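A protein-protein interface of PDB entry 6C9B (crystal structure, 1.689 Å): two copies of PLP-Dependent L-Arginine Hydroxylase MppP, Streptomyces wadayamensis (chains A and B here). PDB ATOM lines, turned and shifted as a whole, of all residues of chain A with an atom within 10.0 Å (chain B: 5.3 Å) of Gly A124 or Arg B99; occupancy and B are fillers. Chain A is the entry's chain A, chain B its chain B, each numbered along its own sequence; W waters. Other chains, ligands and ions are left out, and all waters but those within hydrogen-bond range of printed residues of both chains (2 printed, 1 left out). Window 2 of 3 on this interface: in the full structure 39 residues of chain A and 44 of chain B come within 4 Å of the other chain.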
ATOM      1  N   SER A  91     -18.826 -16.427  -6.922  1.00  0.00           N
ATOM      2  CA  SER A  91     -17.738 -15.531  -6.503  1.00  0.00           C
ATOM      3  C   SER A  91     -17.147 -15.933  -5.155  1.00  0.00           C
ATOM      4  O   SER A  91     -15.956 -15.709  -4.920  1.00  0.00           O
ATOM      5  CB  SER A  91     -18.230 -14.082  -6.447  1.00  0.00           C
ATOM      6  OG  SER A  91     -18.565 -13.630  -7.745  1.00  0.00           O
ATOM      7  N   VAL A  92     -17.958 -16.496  -4.251  1.00  0.00           N
ATOM      8  CA  VAL A  92     -17.394 -17.057  -3.028  1.00  0.00           C
ATOM      9  C   VAL A  92     -16.501 -18.246  -3.367  1.00  0.00           C
ATOM     10  O   VAL A  92     -15.382 -18.369  -2.843  1.00  0.00           O
ATOM     11  CB  VAL A  92     -18.518 -17.435  -2.046  1.00  0.00           C
ATOM     12  CG1 VAL A  92     -17.946 -18.228  -0.905  1.00  0.00           C
ATOM     13  CG2 VAL A  92     -19.226 -16.160  -1.543  1.00  0.00           C
ATOM     14  N   MET A  94     -14.873 -18.558  -6.064  1.00  0.00           N
ATOM     15  CA  MET A  94     -13.688 -17.954  -6.679  1.00  0.00           C
ATOM     16  C   MET A  94     -12.739 -17.355  -5.629  1.00  0.00           C
ATOM     17  O   MET A  94     -11.510 -17.448  -5.755  1.00  0.00           O
ATOM     18  CB  MET A  94     -14.152 -16.901  -7.700  1.00  0.00           C
ATOM     19  CG  MET A  94     -13.028 -16.286  -8.483  1.00  0.00           C
ATOM     20  SD  MET A  94     -12.317 -17.498  -9.652  1.00  0.00           S
ATOM     21  CE  MET A  94     -10.565 -17.247  -9.378  1.00  0.00           C
ATOM     22  N   GLU A  95     -13.289 -16.752  -4.574  1.00  0.00           N
ATOM     23  CA  GLU A  95     -12.455 -16.260  -3.490  1.00  0.00           C
ATOM     24  C   GLU A  95     -11.715 -17.414  -2.823  1.00  0.00           C
ATOM     25  O   GLU A  95     -10.512 -17.314  -2.517  1.00  0.00           O
ATOM     26  CB  GLU A  95     -13.341 -15.511  -2.497  1.00  0.00           C
ATOM     27  CG  GLU A  95     -12.639 -15.041  -1.190  1.00  0.00           C
ATOM     28  CD  GLU A  95     -11.715 -13.875  -1.389  1.00  0.00           C
ATOM     29  OE1 GLU A  95     -11.558 -13.435  -2.550  1.00  0.00           O
ATOM     30  OE2 GLU A  95     -11.142 -13.392  -0.384  1.00  0.00           O
ATOM     31  N   ILE A  96     -12.425 -18.517  -2.580  1.00  0.00           N
ATOM     32  CA  ILE A  96     -11.787 -19.707  -2.026  1.00  0.00           C
ATOM     33  C   ILE A  96     -10.669 -20.180  -2.944  1.00  0.00           C
ATOM     34  O   ILE A  96      -9.557 -20.485  -2.492  1.00  0.00           O
ATOM     35  CB  ILE A  96     -12.850 -20.806  -1.814  1.00  0.00           C
ATOM     36  CG1 ILE A  96     -13.789 -20.417  -0.666  1.00  0.00           C
ATOM     37  CG2 ILE A  96     -12.180 -22.170  -1.515  1.00  0.00           C
ATOM     38  CD1 ILE A  96     -15.104 -21.216  -0.647  1.00  0.00           C
ATOM     39  N   LEU A  97     -10.956 -20.275  -4.249  1.00  0.00           N
ATOM     40  CA  LEU A  97      -9.953 -20.742  -5.203  1.00  0.00           C
ATOM     41  C   LEU A  97      -8.763 -19.794  -5.245  1.00  0.00           C
ATOM     42  O   LEU A  97      -7.610 -20.235  -5.211  1.00  0.00           O
ATOM     43  CB  LEU A  97     -10.558 -20.898  -6.601  1.00  0.00           C
ATOM     44  CG  LEU A  97      -9.577 -21.298  -7.712  1.00  0.00           C
ATOM     45  CD1 LEU A  97      -8.849 -22.601  -7.451  1.00  0.00           C
ATOM     46  CD2 LEU A  97     -10.283 -21.370  -9.048  1.00  0.00           C
ATOM     47  N   ALA A  98      -9.026 -18.483  -5.312  1.00  0.00           N
ATOM     48  CA  ALA A  98      -7.934 -17.518  -5.395  1.00  0.00           C
ATOM     49  C   ALA A  98      -7.052 -17.590  -4.153  1.00  0.00           C
ATOM     50  O   ALA A  98      -5.828 -17.653  -4.252  1.00  0.00           O
ATOM     51  CB  ALA A  98      -8.481 -16.109  -5.574  1.00  0.00           C
ATOM     52  N   ARG A  99      -7.662 -17.622  -2.970  1.00  0.00           N
ATOM     53  CA  ARG A  99      -6.872 -17.763  -1.753  1.00  0.00           C
ATOM     54  C   ARG A  99      -6.106 -19.074  -1.734  1.00  0.00           C
ATOM     55  O   ARG A  99      -4.960 -19.134  -1.246  1.00  0.00           O
ATOM     56  CB  ARG A  99      -7.779 -17.670  -0.533  1.00  0.00           C
ATOM     57  CG  ARG A  99      -8.062 -16.276  -0.172  1.00  0.00           C
ATOM     58  CD  ARG A  99      -7.541 -15.953   1.234  1.00  0.00           C
ATOM     59  NE  ARG A  99      -8.622 -16.211   2.157  1.00  0.00           N
ATOM     60  CZ  ARG A  99      -8.610 -17.108   3.131  1.00  0.00           C
ATOM     61  NH1 ARG A  99      -9.686 -17.204   3.873  1.00  0.00           N
ATOM     62  NH2 ARG A  99      -7.539 -17.860   3.389  1.00  0.00           N
ATOM     63  N   SER A 100      -6.726 -20.138  -2.239  1.00  0.00           N
ATOM     64  CA  SER A 100      -6.084 -21.442  -2.233  1.00  0.00           C
ATOM     65  C   SER A 100      -4.889 -21.490  -3.182  1.00  0.00           C
ATOM     66  O   SER A 100      -3.896 -22.164  -2.897  1.00  0.00           O
ATOM     67  CB  SER A 100      -7.085 -22.526  -2.620  1.00  0.00           C
ATOM     68  OG  SER A 100      -8.112 -22.671  -1.641  1.00  0.00           O
ATOM     69  N   SER A 102      -2.947 -18.889  -3.822  1.00  0.00           N
ATOM     70  CA  SER A 102      -1.949 -17.851  -3.550  1.00  0.00           C
ATOM     71  C   SER A 102      -0.684 -18.361  -2.857  1.00  0.00           C
ATOM     72  O   SER A 102       0.386 -17.781  -3.058  1.00  0.00           O
ATOM     73  CB  SER A 102      -2.593 -16.719  -2.733  1.00  0.00           C
ATOM     74  OG  SER A 102      -2.850 -17.144  -1.429  1.00  0.00           O
ATOM     75  N   ASP A 116     -14.928  -9.416 -15.071  1.00  0.00           N
ATOM     76  CA  ASP A 116     -13.790  -8.763 -14.422  1.00  0.00           C
ATOM     77  C   ASP A 116     -13.641  -9.142 -12.948  1.00  0.00           C
ATOM     78  O   ASP A 116     -12.536  -9.011 -12.401  1.00  0.00           O
ATOM     79  CB  ASP A 116     -13.878  -7.239 -14.568  1.00  0.00           C
ATOM     80  CG  ASP A 116     -15.183  -6.672 -14.056  1.00  0.00           C
ATOM     81  OD1 ASP A 116     -16.252  -7.101 -14.541  1.00  0.00           O
ATOM     82  OD2 ASP A 116     -15.135  -5.789 -13.177  1.00  0.00           O
ATOM     83  N   ASN A 117     -14.700  -9.608 -12.290  1.00  0.00           N
ATOM     84  CA  ASN A 117     -14.576 -10.052 -10.905  1.00  0.00           C
ATOM     85  C   ASN A 117     -13.520 -11.131 -10.757  1.00  0.00           C
ATOM     86  O   ASN A 117     -12.854 -11.220  -9.721  1.00  0.00           O
ATOM     87  CB  ASN A 117     -15.912 -10.614 -10.391  1.00  0.00           C
ATOM     88  CG  ASN A 117     -16.840  -9.547  -9.854  1.00  0.00           C
ATOM     89  OD1 ASN A 117     -16.615  -8.999  -8.776  1.00  0.00           O
ATOM     90  ND2 ASN A 117     -17.911  -9.272 -10.587  1.00  0.00           N
ATOM     91  N   ILE A 118     -13.390 -12.007 -11.753  1.00  0.00           N
ATOM     92  CA  ILE A 118     -12.401 -13.082 -11.655  1.00  0.00           C
ATOM     93  C   ILE A 118     -11.003 -12.489 -11.562  1.00  0.00           C
ATOM     94  O   ILE A 118     -10.186 -12.882 -10.714  1.00  0.00           O
ATOM     95  CB  ILE A 118     -12.526 -14.050 -12.844  1.00  0.00           C
ATOM     96  CG1 ILE A 118     -13.908 -14.736 -12.830  1.00  0.00           C
ATOM     97  CG2 ILE A 118     -11.406 -15.081 -12.814  1.00  0.00           C
ATOM     98  CD1 ILE A 118     -14.315 -15.371 -14.158  1.00  0.00           C
ATOM     99  N   ALA A 119     -10.703 -11.532 -12.439  1.00  0.00           N
ATOM    100  CA  ALA A 119      -9.414 -10.865 -12.385  1.00  0.00           C
ATOM    101  C   ALA A 119      -9.220 -10.128 -11.069  1.00  0.00           C
ATOM    102  O   ALA A 119      -8.127 -10.166 -10.491  1.00  0.00           O
ATOM    103  CB  ALA A 119      -9.283  -9.898 -13.556  1.00  0.00           C
ATOM    104  N   ASP A 120     -10.268  -9.449 -10.572  1.00  0.00           N
ATOM    105  CA  ASP A 120     -10.101  -8.653  -9.356  1.00  0.00           C
ATOM    106  C   ASP A 120      -9.943  -9.542  -8.123  1.00  0.00           C
ATOM    107  O   ASP A 120      -9.183  -9.185  -7.214  1.00  0.00           O
ATOM    108  CB  ASP A 120     -11.279  -7.691  -9.154  1.00  0.00           C
ATOM    109  CG  ASP A 120     -11.293  -6.560 -10.183  1.00  0.00           C
ATOM    110  OD1 ASP A 120     -10.236  -6.299 -10.784  1.00  0.00           O
ATOM    111  OD2 ASP A 120     -12.356  -5.943 -10.364  1.00  0.00           O
ATOM    112  N   LEU A 121     -10.603 -10.706  -8.099  1.00  0.00           N
ATOM    113  CA  LEU A 121     -10.420 -11.646  -6.989  1.00  0.00           C
ATOM    114  C   LEU A 121      -9.037 -12.290  -7.046  1.00  0.00           C
ATOM    115  O   LEU A 121      -8.379 -12.451  -6.013  1.00  0.00           O
ATOM    116  CB  LEU A 121     -11.523 -12.699  -6.991  1.00  0.00           C
ATOM    117  CG  LEU A 121     -12.903 -12.180  -6.577  1.00  0.00           C
ATOM    118  CD1 LEU A 121     -13.962 -13.282  -6.745  1.00  0.00           C
ATOM    119  CD2 LEU A 121     -12.943 -11.654  -5.163  1.00  0.00           C
ATOM    120  N   LEU A 122      -8.558 -12.632  -8.238  1.00  0.00           N
ATOM    121  CA  LEU A 122      -7.210 -13.188  -8.326  1.00  0.00           C
ATOM    122  C   LEU A 122      -6.160 -12.150  -7.938  1.00  0.00           C
ATOM    123  O   LEU A 122      -5.287 -12.412  -7.102  1.00  0.00           O
ATOM    124  CB  LEU A 122      -6.956 -13.721  -9.736  1.00  0.00           C
ATOM    125  CG  LEU A 122      -7.691 -15.005 -10.097  1.00  0.00           C
ATOM    126  CD1 LEU A 122      -7.633 -15.263 -11.620  1.00  0.00           C
ATOM    127  CD2 LEU A 122      -7.145 -16.205  -9.305  1.00  0.00           C
ATOM    128  N   ARG A 123      -6.231 -10.955  -8.534  1.00  0.00           N
ATOM    129  CA  ARG A 123      -5.268  -9.916  -8.209  1.00  0.00           C
ATOM    130  C   ARG A 123      -5.332  -9.529  -6.742  1.00  0.00           C
ATOM    131  O   ARG A 123      -4.294  -9.252  -6.125  1.00  0.00           O
ATOM    132  CB  ARG A 123      -5.509  -8.683  -9.068  1.00  0.00           C
ATOM    133  CG  ARG A 123      -5.101  -8.847 -10.513  1.00  0.00           C
ATOM    134  CD  ARG A 123      -4.746  -7.475 -11.057  1.00  0.00           C
ATOM    135  NE  ARG A 123      -5.024  -7.313 -12.474  1.00  0.00           N
ATOM    136  CZ  ARG A 123      -6.182  -6.883 -12.968  1.00  0.00           C
ATOM    137  NH1 ARG A 123      -7.201  -6.590 -12.169  1.00  0.00           N
ATOM    138  NH2 ARG A 123      -6.321  -6.758 -14.273  1.00  0.00           N
ATOM    139  N   GLY A 124      -6.541  -9.448  -6.179  1.00  0.00           N
ATOM    140  CA  GLY A 124      -6.700  -9.058  -4.790  1.00  0.00           C
ATOM    141  C   GLY A 124      -6.102 -10.047  -3.822  1.00  0.00           C
ATOM    142  O   GLY A 124      -5.784  -9.685  -2.692  1.00  0.00           O
ATOM    143  N   ASN A 125      -5.956 -11.295  -4.239  1.00  0.00           N
ATOM    144  CA  ASN A 125      -5.294 -12.316  -3.442  1.00  0.00           C
ATOM    145  C   ASN A 125      -3.826 -12.504  -3.822  1.00  0.00           C
ATOM    146  O   ASN A 125      -3.214 -13.504  -3.439  1.00  0.00           O
ATOM    147  CB  ASN A 125      -6.083 -13.616  -3.569  1.00  0.00           C
ATOM    148  CG  ASN A 125      -7.321 -13.611  -2.707  1.00  0.00           C
ATOM    149  OD1 ASN A 125      -7.218 -13.771  -1.496  1.00  0.00           O
ATOM    150  ND2 ASN A 125      -8.485 -13.377  -3.308  1.00  0.00           N
ATOM    151  N   GLY A 126      -3.238 -11.564  -4.562  1.00  0.00           N
ATOM    152  CA  GLY A 126      -1.808 -11.580  -4.777  1.00  0.00           C
ATOM    153  C   GLY A 126      -1.334 -12.287  -6.022  1.00  0.00           C
ATOM    154  O   GLY A 126      -0.125 -12.433  -6.211  1.00  0.00           O
ATOM    155  N   LEU A 127      -2.228 -12.708  -6.898  1.00  0.00           N
ATOM    156  CA  LEU A 127      -1.810 -13.422  -8.095  1.00  0.00           C
ATOM    157  C   LEU A 127      -1.581 -12.436  -9.233  1.00  0.00           C
ATOM    158  O   LEU A 127      -2.318 -11.465  -9.390  1.00  0.00           O
ATOM    159  CB  LEU A 127      -2.870 -14.450  -8.455  1.00  0.00           C
ATOM    160  CG  LEU A 127      -2.838 -15.470  -7.299  1.00  0.00           C
ATOM    161  CD1 LEU A 127      -4.175 -15.767  -6.737  1.00  0.00           C
ATOM    162  CD2 LEU A 127      -2.069 -16.684  -7.717  1.00  0.00           C
ATOM    163  N   ASP A 128      -0.526 -12.671 -10.002  1.00  0.00           N
ATOM    164  CA  ASP A 128      -0.268 -11.902 -11.208  1.00  0.00           C
ATOM    165  C   ASP A 128      -0.942 -12.597 -12.380  1.00  0.00           C
ATOM    166  O   ASP A 128      -0.975 -13.829 -12.440  1.00  0.00           O
ATOM    167  CB  ASP A 128       1.229 -11.787 -11.453  1.00  0.00           C
ATOM    168  CG  ASP A 128       1.915 -10.896 -10.435  1.00  0.00           C
ATOM    169  OD1 ASP A 128       1.304  -9.889 -10.022  1.00  0.00           O
ATOM    170  OD2 ASP A 128       3.061 -11.207 -10.050  1.00  0.00           O
ATOM    171  N   LEU A 129      -1.484 -11.807 -13.297  1.00  0.00           N
ATOM    172  CA  LEU A 129      -2.303 -12.321 -14.386  1.00  0.00           C
ATOM    173  C   LEU A 129      -1.593 -12.172 -15.719  1.00  0.00           C
ATOM    174  O   LEU A 129      -0.980 -11.134 -16.007  1.00  0.00           O
ATOM    175  CB  LEU A 129      -3.643 -11.591 -14.466  1.00  0.00           C
ATOM    176  CG  LEU A 129      -4.441 -11.643 -13.173  1.00  0.00           C
ATOM    177  CD1 LEU A 129      -5.773 -10.897 -13.351  1.00  0.00           C
ATOM    178  CD2 LEU A 129      -4.679 -13.077 -12.744  1.00  0.00           C
ATOM    179  N   ILE A 246     -10.056 -24.026   3.191  1.00  0.00           N
ATOM    180  CA  ILE A 246     -10.523 -22.645   3.149  1.00  0.00           C
ATOM    181  C   ILE A 246     -12.032 -22.581   2.989  1.00  0.00           C
ATOM    182  O   ILE A 246     -12.689 -21.714   3.576  1.00  0.00           O
ATOM    183  CB  ILE A 246      -9.770 -21.870   2.051  1.00  0.00           C
ATOM    184  CG1 ILE A 246      -8.301 -21.777   2.467  1.00  0.00           C
ATOM    185  CG2 ILE A 246     -10.394 -20.480   1.852  1.00  0.00           C
ATOM    186  CD1 ILE A 246      -7.395 -21.172   1.394  1.00  0.00           C
ATOM    187  N   ILE A 250     -14.878 -20.685   5.724  1.00  0.00           N
ATOM    188  CA  ILE A 250     -15.897 -19.724   5.337  1.00  0.00           C
ATOM    189  C   ILE A 250     -17.295 -20.230   5.640  1.00  0.00           C
ATOM    190  O   ILE A 250     -18.124 -19.448   6.093  1.00  0.00           O
ATOM    191  CB  ILE A 250     -15.741 -19.342   3.858  1.00  0.00           C
ATOM    192  CG1 ILE A 250     -14.401 -18.607   3.665  1.00  0.00           C
ATOM    193  CG2 ILE A 250     -16.908 -18.484   3.380  1.00  0.00           C
ATOM    194  CD1 ILE A 250     -14.109 -18.222   2.267  1.00  0.00           C
ATOM    195  N   MET B  94     -16.499 -11.447   7.447  1.00  0.00           N
ATOM    196  CA  MET B  94     -15.193 -11.575   8.086  1.00  0.00           C
ATOM    197  C   MET B  94     -14.080 -11.767   7.051  1.00  0.00           C
ATOM    198  O   MET B  94     -12.974 -11.254   7.223  1.00  0.00           O
ATOM    199  CB  MET B  94     -15.234 -12.737   9.090  1.00  0.00           C
ATOM    200  CG  MET B  94     -13.953 -12.941   9.852  1.00  0.00           C
ATOM    201  SD  MET B  94     -13.773 -11.601  11.045  1.00  0.00           S
ATOM    202  CE  MET B  94     -12.008 -11.333  10.885  1.00  0.00           C
ATOM    203  N   GLU B  95     -14.341 -12.517   5.979  1.00  0.00           N
ATOM    204  CA  GLU B  95     -13.357 -12.645   4.912  1.00  0.00           C
ATOM    205  C   GLU B  95     -13.070 -11.287   4.291  1.00  0.00           C
ATOM    206  O   GLU B  95     -11.912 -10.942   4.023  1.00  0.00           O
ATOM    207  CB  GLU B  95     -13.844 -13.633   3.852  1.00  0.00           C
ATOM    208  CG  GLU B  95     -12.971 -13.727   2.614  1.00  0.00           C
ATOM    209  CD  GLU B  95     -11.632 -14.428   2.790  1.00  0.00           C
ATOM    210  OE1 GLU B  95     -11.280 -14.836   3.903  1.00  0.00           O
ATOM    211  OE2 GLU B  95     -10.900 -14.565   1.776  1.00  0.00           O
ATOM    212  N   ILE B  96     -14.119 -10.509   4.051  1.00  0.00           N
ATOM    213  CA  ILE B  96     -13.951  -9.170   3.490  1.00  0.00           C
ATOM    214  C   ILE B  96     -13.118  -8.315   4.433  1.00  0.00           C
ATOM    215  O   ILE B  96     -12.178  -7.625   4.009  1.00  0.00           O
ATOM    216  CB  ILE B  96     -15.333  -8.551   3.214  1.00  0.00           C
ATOM    217  CG1 ILE B  96     -16.023  -9.288   2.068  1.00  0.00           C
ATOM    218  CG2 ILE B  96     -15.211  -7.074   2.889  1.00  0.00           C
ATOM    219  CD1 ILE B  96     -17.516  -9.011   1.982  1.00  0.00           C
ATOM    220  N   LEU B  97     -13.453  -8.346   5.729  1.00  0.00           N
ATOM    221  CA  LEU B  97     -12.730  -7.534   6.701  1.00  0.00           C
ATOM    222  C   LEU B  97     -11.275  -7.972   6.784  1.00  0.00           C
ATOM    223  O   LEU B  97     -10.362  -7.149   6.890  1.00  0.00           O
ATOM    224  CB  LEU B  97     -13.409  -7.633   8.068  1.00  0.00           C
ATOM    225  CG  LEU B  97     -12.710  -6.937   9.243  1.00  0.00           C
ATOM    226  CD1 LEU B  97     -12.576  -5.444   8.973  1.00  0.00           C
ATOM    227  CD2 LEU B  97     -13.456  -7.191  10.559  1.00  0.00           C
ATOM    228  N   ALA B  98     -11.045  -9.269   6.801  1.00  0.00           N
ATOM    229  CA  ALA B  98      -9.683  -9.760   6.967  1.00  0.00           C
ATOM    230  C   ALA B  98      -8.828  -9.365   5.768  1.00  0.00           C
ATOM    231  O   ALA B  98      -7.689  -8.914   5.927  1.00  0.00           O
ATOM    232  CB  ALA B  98      -9.708 -11.273   7.146  1.00  0.00           C
ATOM    233  N   ARG B  99      -9.342  -9.584   4.552  1.00  0.00           N
ATOM    234  CA  ARG B  99      -8.563  -9.214   3.378  1.00  0.00           C
ATOM    235  C   ARG B  99      -8.368  -7.704   3.337  1.00  0.00           C
ATOM    236  O   ARG B  99      -7.296  -7.229   2.944  1.00  0.00           O
ATOM    237  CB  ARG B  99      -9.230  -9.739   2.104  1.00  0.00           C
ATOM    238  CG  ARG B  99      -8.305  -9.553   0.881  1.00  0.00           C
ATOM    239  CD  ARG B  99      -8.289 -10.775  -0.003  1.00  0.00           C
ATOM    240  NE  ARG B  99      -9.510 -10.983  -0.764  1.00  0.00           N
ATOM    241  CZ  ARG B  99      -9.884 -10.238  -1.797  1.00  0.00           C
ATOM    242  NH1 ARG B  99     -10.980 -10.559  -2.463  1.00  0.00           N
ATOM    243  NH2 ARG B  99      -9.188  -9.156  -2.142  1.00  0.00           N
ATOM    244  N   SER B 100      -9.369  -6.940   3.807  1.00  0.00           N
ATOM    245  CA  SER B 100      -9.243  -5.482   3.855  1.00  0.00           C
ATOM    246  C   SER B 100      -8.190  -5.048   4.868  1.00  0.00           C
ATOM    247  O   SER B 100      -7.392  -4.140   4.593  1.00  0.00           O
ATOM    248  CB  SER B 100     -10.574  -4.846   4.213  1.00  0.00           C
ATOM    249  OG  SER B 100     -11.534  -5.092   3.194  1.00  0.00           O
ATOM    250  N   LEU B 101      -8.200  -5.656   6.056  1.00  0.00           N
ATOM    251  CA  LEU B 101      -7.178  -5.356   7.058  1.00  0.00           C
ATOM    252  C   LEU B 101      -5.779  -5.600   6.522  1.00  0.00           C
ATOM    253  O   LEU B 101      -4.853  -4.844   6.835  1.00  0.00           O
ATOM    254  CB  LEU B 101      -7.404  -6.200   8.312  1.00  0.00           C
ATOM    255  CG  LEU B 101      -8.519  -5.732   9.234  1.00  0.00           C
ATOM    256  CD1 LEU B 101      -8.855  -6.846  10.222  1.00  0.00           C
ATOM    257  CD2 LEU B 101      -8.090  -4.480   9.993  1.00  0.00           C
ATOM    258  N   SER B 102      -5.596  -6.673   5.747  1.00  0.00           N
ATOM    259  CA  SER B 102      -4.265  -7.071   5.305  1.00  0.00           C
ATOM    260  C   SER B 102      -3.628  -6.014   4.416  1.00  0.00           C
ATOM    261  O   SER B 102      -2.404  -6.028   4.240  1.00  0.00           O
ATOM    262  CB  SER B 102      -4.324  -8.428   4.577  1.00  0.00           C
ATOM    263  OG  SER B 102      -4.777  -8.295   3.235  1.00  0.00           O
ATOM    264  N   ALA B 103      -4.423  -5.070   3.896  1.00  0.00           N
ATOM    265  CA  ALA B 103      -3.879  -3.988   3.077  1.00  0.00           C
ATOM    266  C   ALA B 103      -2.992  -3.042   3.878  1.00  0.00           C
ATOM    267  O   ALA B 103      -2.080  -2.433   3.308  1.00  0.00           O
ATOM    268  CB  ALA B 103      -5.014  -3.184   2.435  1.00  0.00           C
ATOM    269  N   ASN B 125      -5.429 -14.629   5.689  1.00  0.00           N
ATOM    270  CA  ASN B 125      -5.176 -13.422   4.925  1.00  0.00           C
ATOM    271  C   ASN B 125      -3.898 -12.719   5.357  1.00  0.00           C
ATOM    272  O   ASN B 125      -3.677 -11.568   4.968  1.00  0.00           O
ATOM    273  CB  ASN B 125      -6.379 -12.502   5.058  1.00  0.00           C
ATOM    274  CG  ASN B 125      -7.516 -12.935   4.164  1.00  0.00           C
ATOM    275  OD1 ASN B 125      -7.464 -12.685   2.961  1.00  0.00           O
ATOM    276  ND2 ASN B 125      -8.493 -13.611   4.712  1.00  0.00           N
ATOM    277  N   ILE B 246     -13.681  -4.478  -1.662  1.00  0.00           N
ATOM    278  CA  ILE B 246     -13.571  -5.930  -1.622  1.00  0.00           C
ATOM    279  C   ILE B 246     -14.962  -6.556  -1.537  1.00  0.00           C
ATOM    280  O   ILE B 246     -15.246  -7.543  -2.223  1.00  0.00           O
ATOM    281  CB  ILE B 246     -12.646  -6.382  -0.486  1.00  0.00           C
ATOM    282  CG1 ILE B 246     -11.212  -5.957  -0.843  1.00  0.00           C
ATOM    283  CG2 ILE B 246     -12.716  -7.913  -0.297  1.00  0.00           C
ATOM    284  CD1 ILE B 246     -10.162  -6.179   0.275  1.00  0.00           C
ATOM    285  N   ASP B 249     -16.192  -6.837  -4.962  1.00  0.00           N
ATOM    286  CA  ASP B 249     -15.558  -7.902  -5.732  1.00  0.00           C
ATOM    287  C   ASP B 249     -16.213  -9.248  -5.458  1.00  0.00           C
ATOM    288  O   ASP B 249     -16.165 -10.137  -6.317  1.00  0.00           O
ATOM    289  CB  ASP B 249     -14.066  -8.002  -5.384  1.00  0.00           C
ATOM    290  CG  ASP B 249     -13.250  -6.811  -5.859  1.00  0.00           C
ATOM    291  OD1 ASP B 249     -13.686  -6.072  -6.769  1.00  0.00           O
ATOM    292  OD2 ASP B 249     -12.121  -6.641  -5.346  1.00  0.00           O
ATOM    293  N   ILE B 250     -16.818  -9.414  -4.290  1.00  0.00           N
ATOM    294  CA  ILE B 250     -17.402 -10.703  -3.905  1.00  0.00           C
ATOM    295  C   ILE B 250     -18.884 -10.778  -4.248  1.00  0.00           C
ATOM    296  O   ILE B 250     -19.367 -11.843  -4.641  1.00  0.00           O
ATOM    297  CB  ILE B 250     -17.145 -10.984  -2.409  1.00  0.00           C
ATOM    298  CG1 ILE B 250     -15.639 -11.196  -2.208  1.00  0.00           C
ATOM    299  CG2 ILE B 250     -17.917 -12.245  -1.935  1.00  0.00           C
ATOM    300  CD1 ILE B 250     -15.213 -11.392  -0.815  1.00  0.00           C
HETATM  301  O   HOH W   1      -7.014  -7.420  -1.594  1.00  0.00           O
HETATM  302  O   HOH W   2     -10.561  -8.670  -4.634  1.00  0.00           O
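The side-chain carboxylate of Glu A95 sits close to the side-chain carboxylate of Glu B95 (2.5 Å). The guanidinium group of Arg B99 is in salt-bridge range of the side-chain carboxylate of Glu A95, at 2.9 Å. The guanidinium group (NE) of Arg A99 lies within salt-bridge range of the side-chain carboxylate (OE2) of Glu B95 (2.8 Å). The side-chain amide oxygen of Asn A117 lies close to the backbone carbonyl oxygen of Asp B249 (2.7 Å). NH2 of Arg B99 sits at hydrogen-bond distance from O of Gly A124, at 3.5 Å.
OE1 of Glu A95 sits at hydrogen-bond distance from ND2 of Asn A125, 3.2 Å away. The side-chain hydroxyl of Ser A102 sits at hydrogen-bond distance from the backbone carbonyl oxygen of Arg A99 (2.9 Å). OD1 of Asp A120 is in salt-bridge range of NH1 of Arg A123 (3.3 Å). The backbone carbonyl oxygen of Leu A121 lies within hydrogen-bond range of the side-chain amide nitrogen of Asn A125 (2.9 Å). The side-chain amide nitrogen (ND2) of Asn B125 sits at hydrogen-bond distance from the side-chain carboxylate (OE1) of Glu B95, 3.1 Å away. The backbone carbonyl oxygen (O) of Arg B99 sits at hydrogen-bond distance from the side-chain hydroxyl (OG) of Ser B102 (2.8 Å).
Ile B250 touches Ser A91 (O to CB, 3.1 Å). NE of Arg A99 touches ND2 of Asn B125, at 3.6 Å. CB of Asp A120 touches OD1 of Asp B249, 3.8 Å away. Leu A121 touches Arg B99. Leu A121 touches Asp B249. Asn A125 touches Arg B99.
Of the printed residues of chain B, Glu A95 touches Glu B95 (2.5 Å) and Arg B99 (2.9 Å). Of chain B, only Arg B99 comes within 4 Å of Gly A124. Ala B98 touches none of the printed residues of chain A. Of the printed residues of chain A, Ile B250 touches Ser A91 (3.1 Å). The nearest printed residue of chain B that does not touch Gly A124 is Asp B249 (6.0 Å). The nearest residue of chain A that does not touch Arg B99 is Asp A120 (5.1 Å).
Of the 26 printed residues of chain A, 8 touch a printed residue of chain B. Hydrophobic or aromatic side chains of chain A that line the printed part of chain B: Leu A121. Along chain A the printed residues that touch a printed residue of chain B span positions 91 to 125. Among the printed residues, Asp or Glu carboxylates within 4 Å of a Lys or Arg side-chain nitrogen of the other chain: Glu A95 with Arg B99 and Arg A99 with Glu B95.
Glu B95 touches its own counterpart, Glu A95. Glu A95 touches Arg B99, and with the chains exchanged Arg A99 touches Glu B95. Arg A99 touches Asn B125, and with the chains exchanged Asn A125 touches Arg B99. Of the 11 pairs that touch across the chains among the printed residues, 5 have their exchanged pair printed and touching as well.
Water W2 lies within hydrogen-bond range of OD2 of Asp B249 (2.7 Å), NH2 of Arg B99 (2.9 Å) and O of Asp A120 (3.0 Å). Water W1 bridges the backbone carbonyl oxygen (O) of Gly A124 (2.8 Å) and the guanidinium group (NH2) of Arg B99 (2.8 Å).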
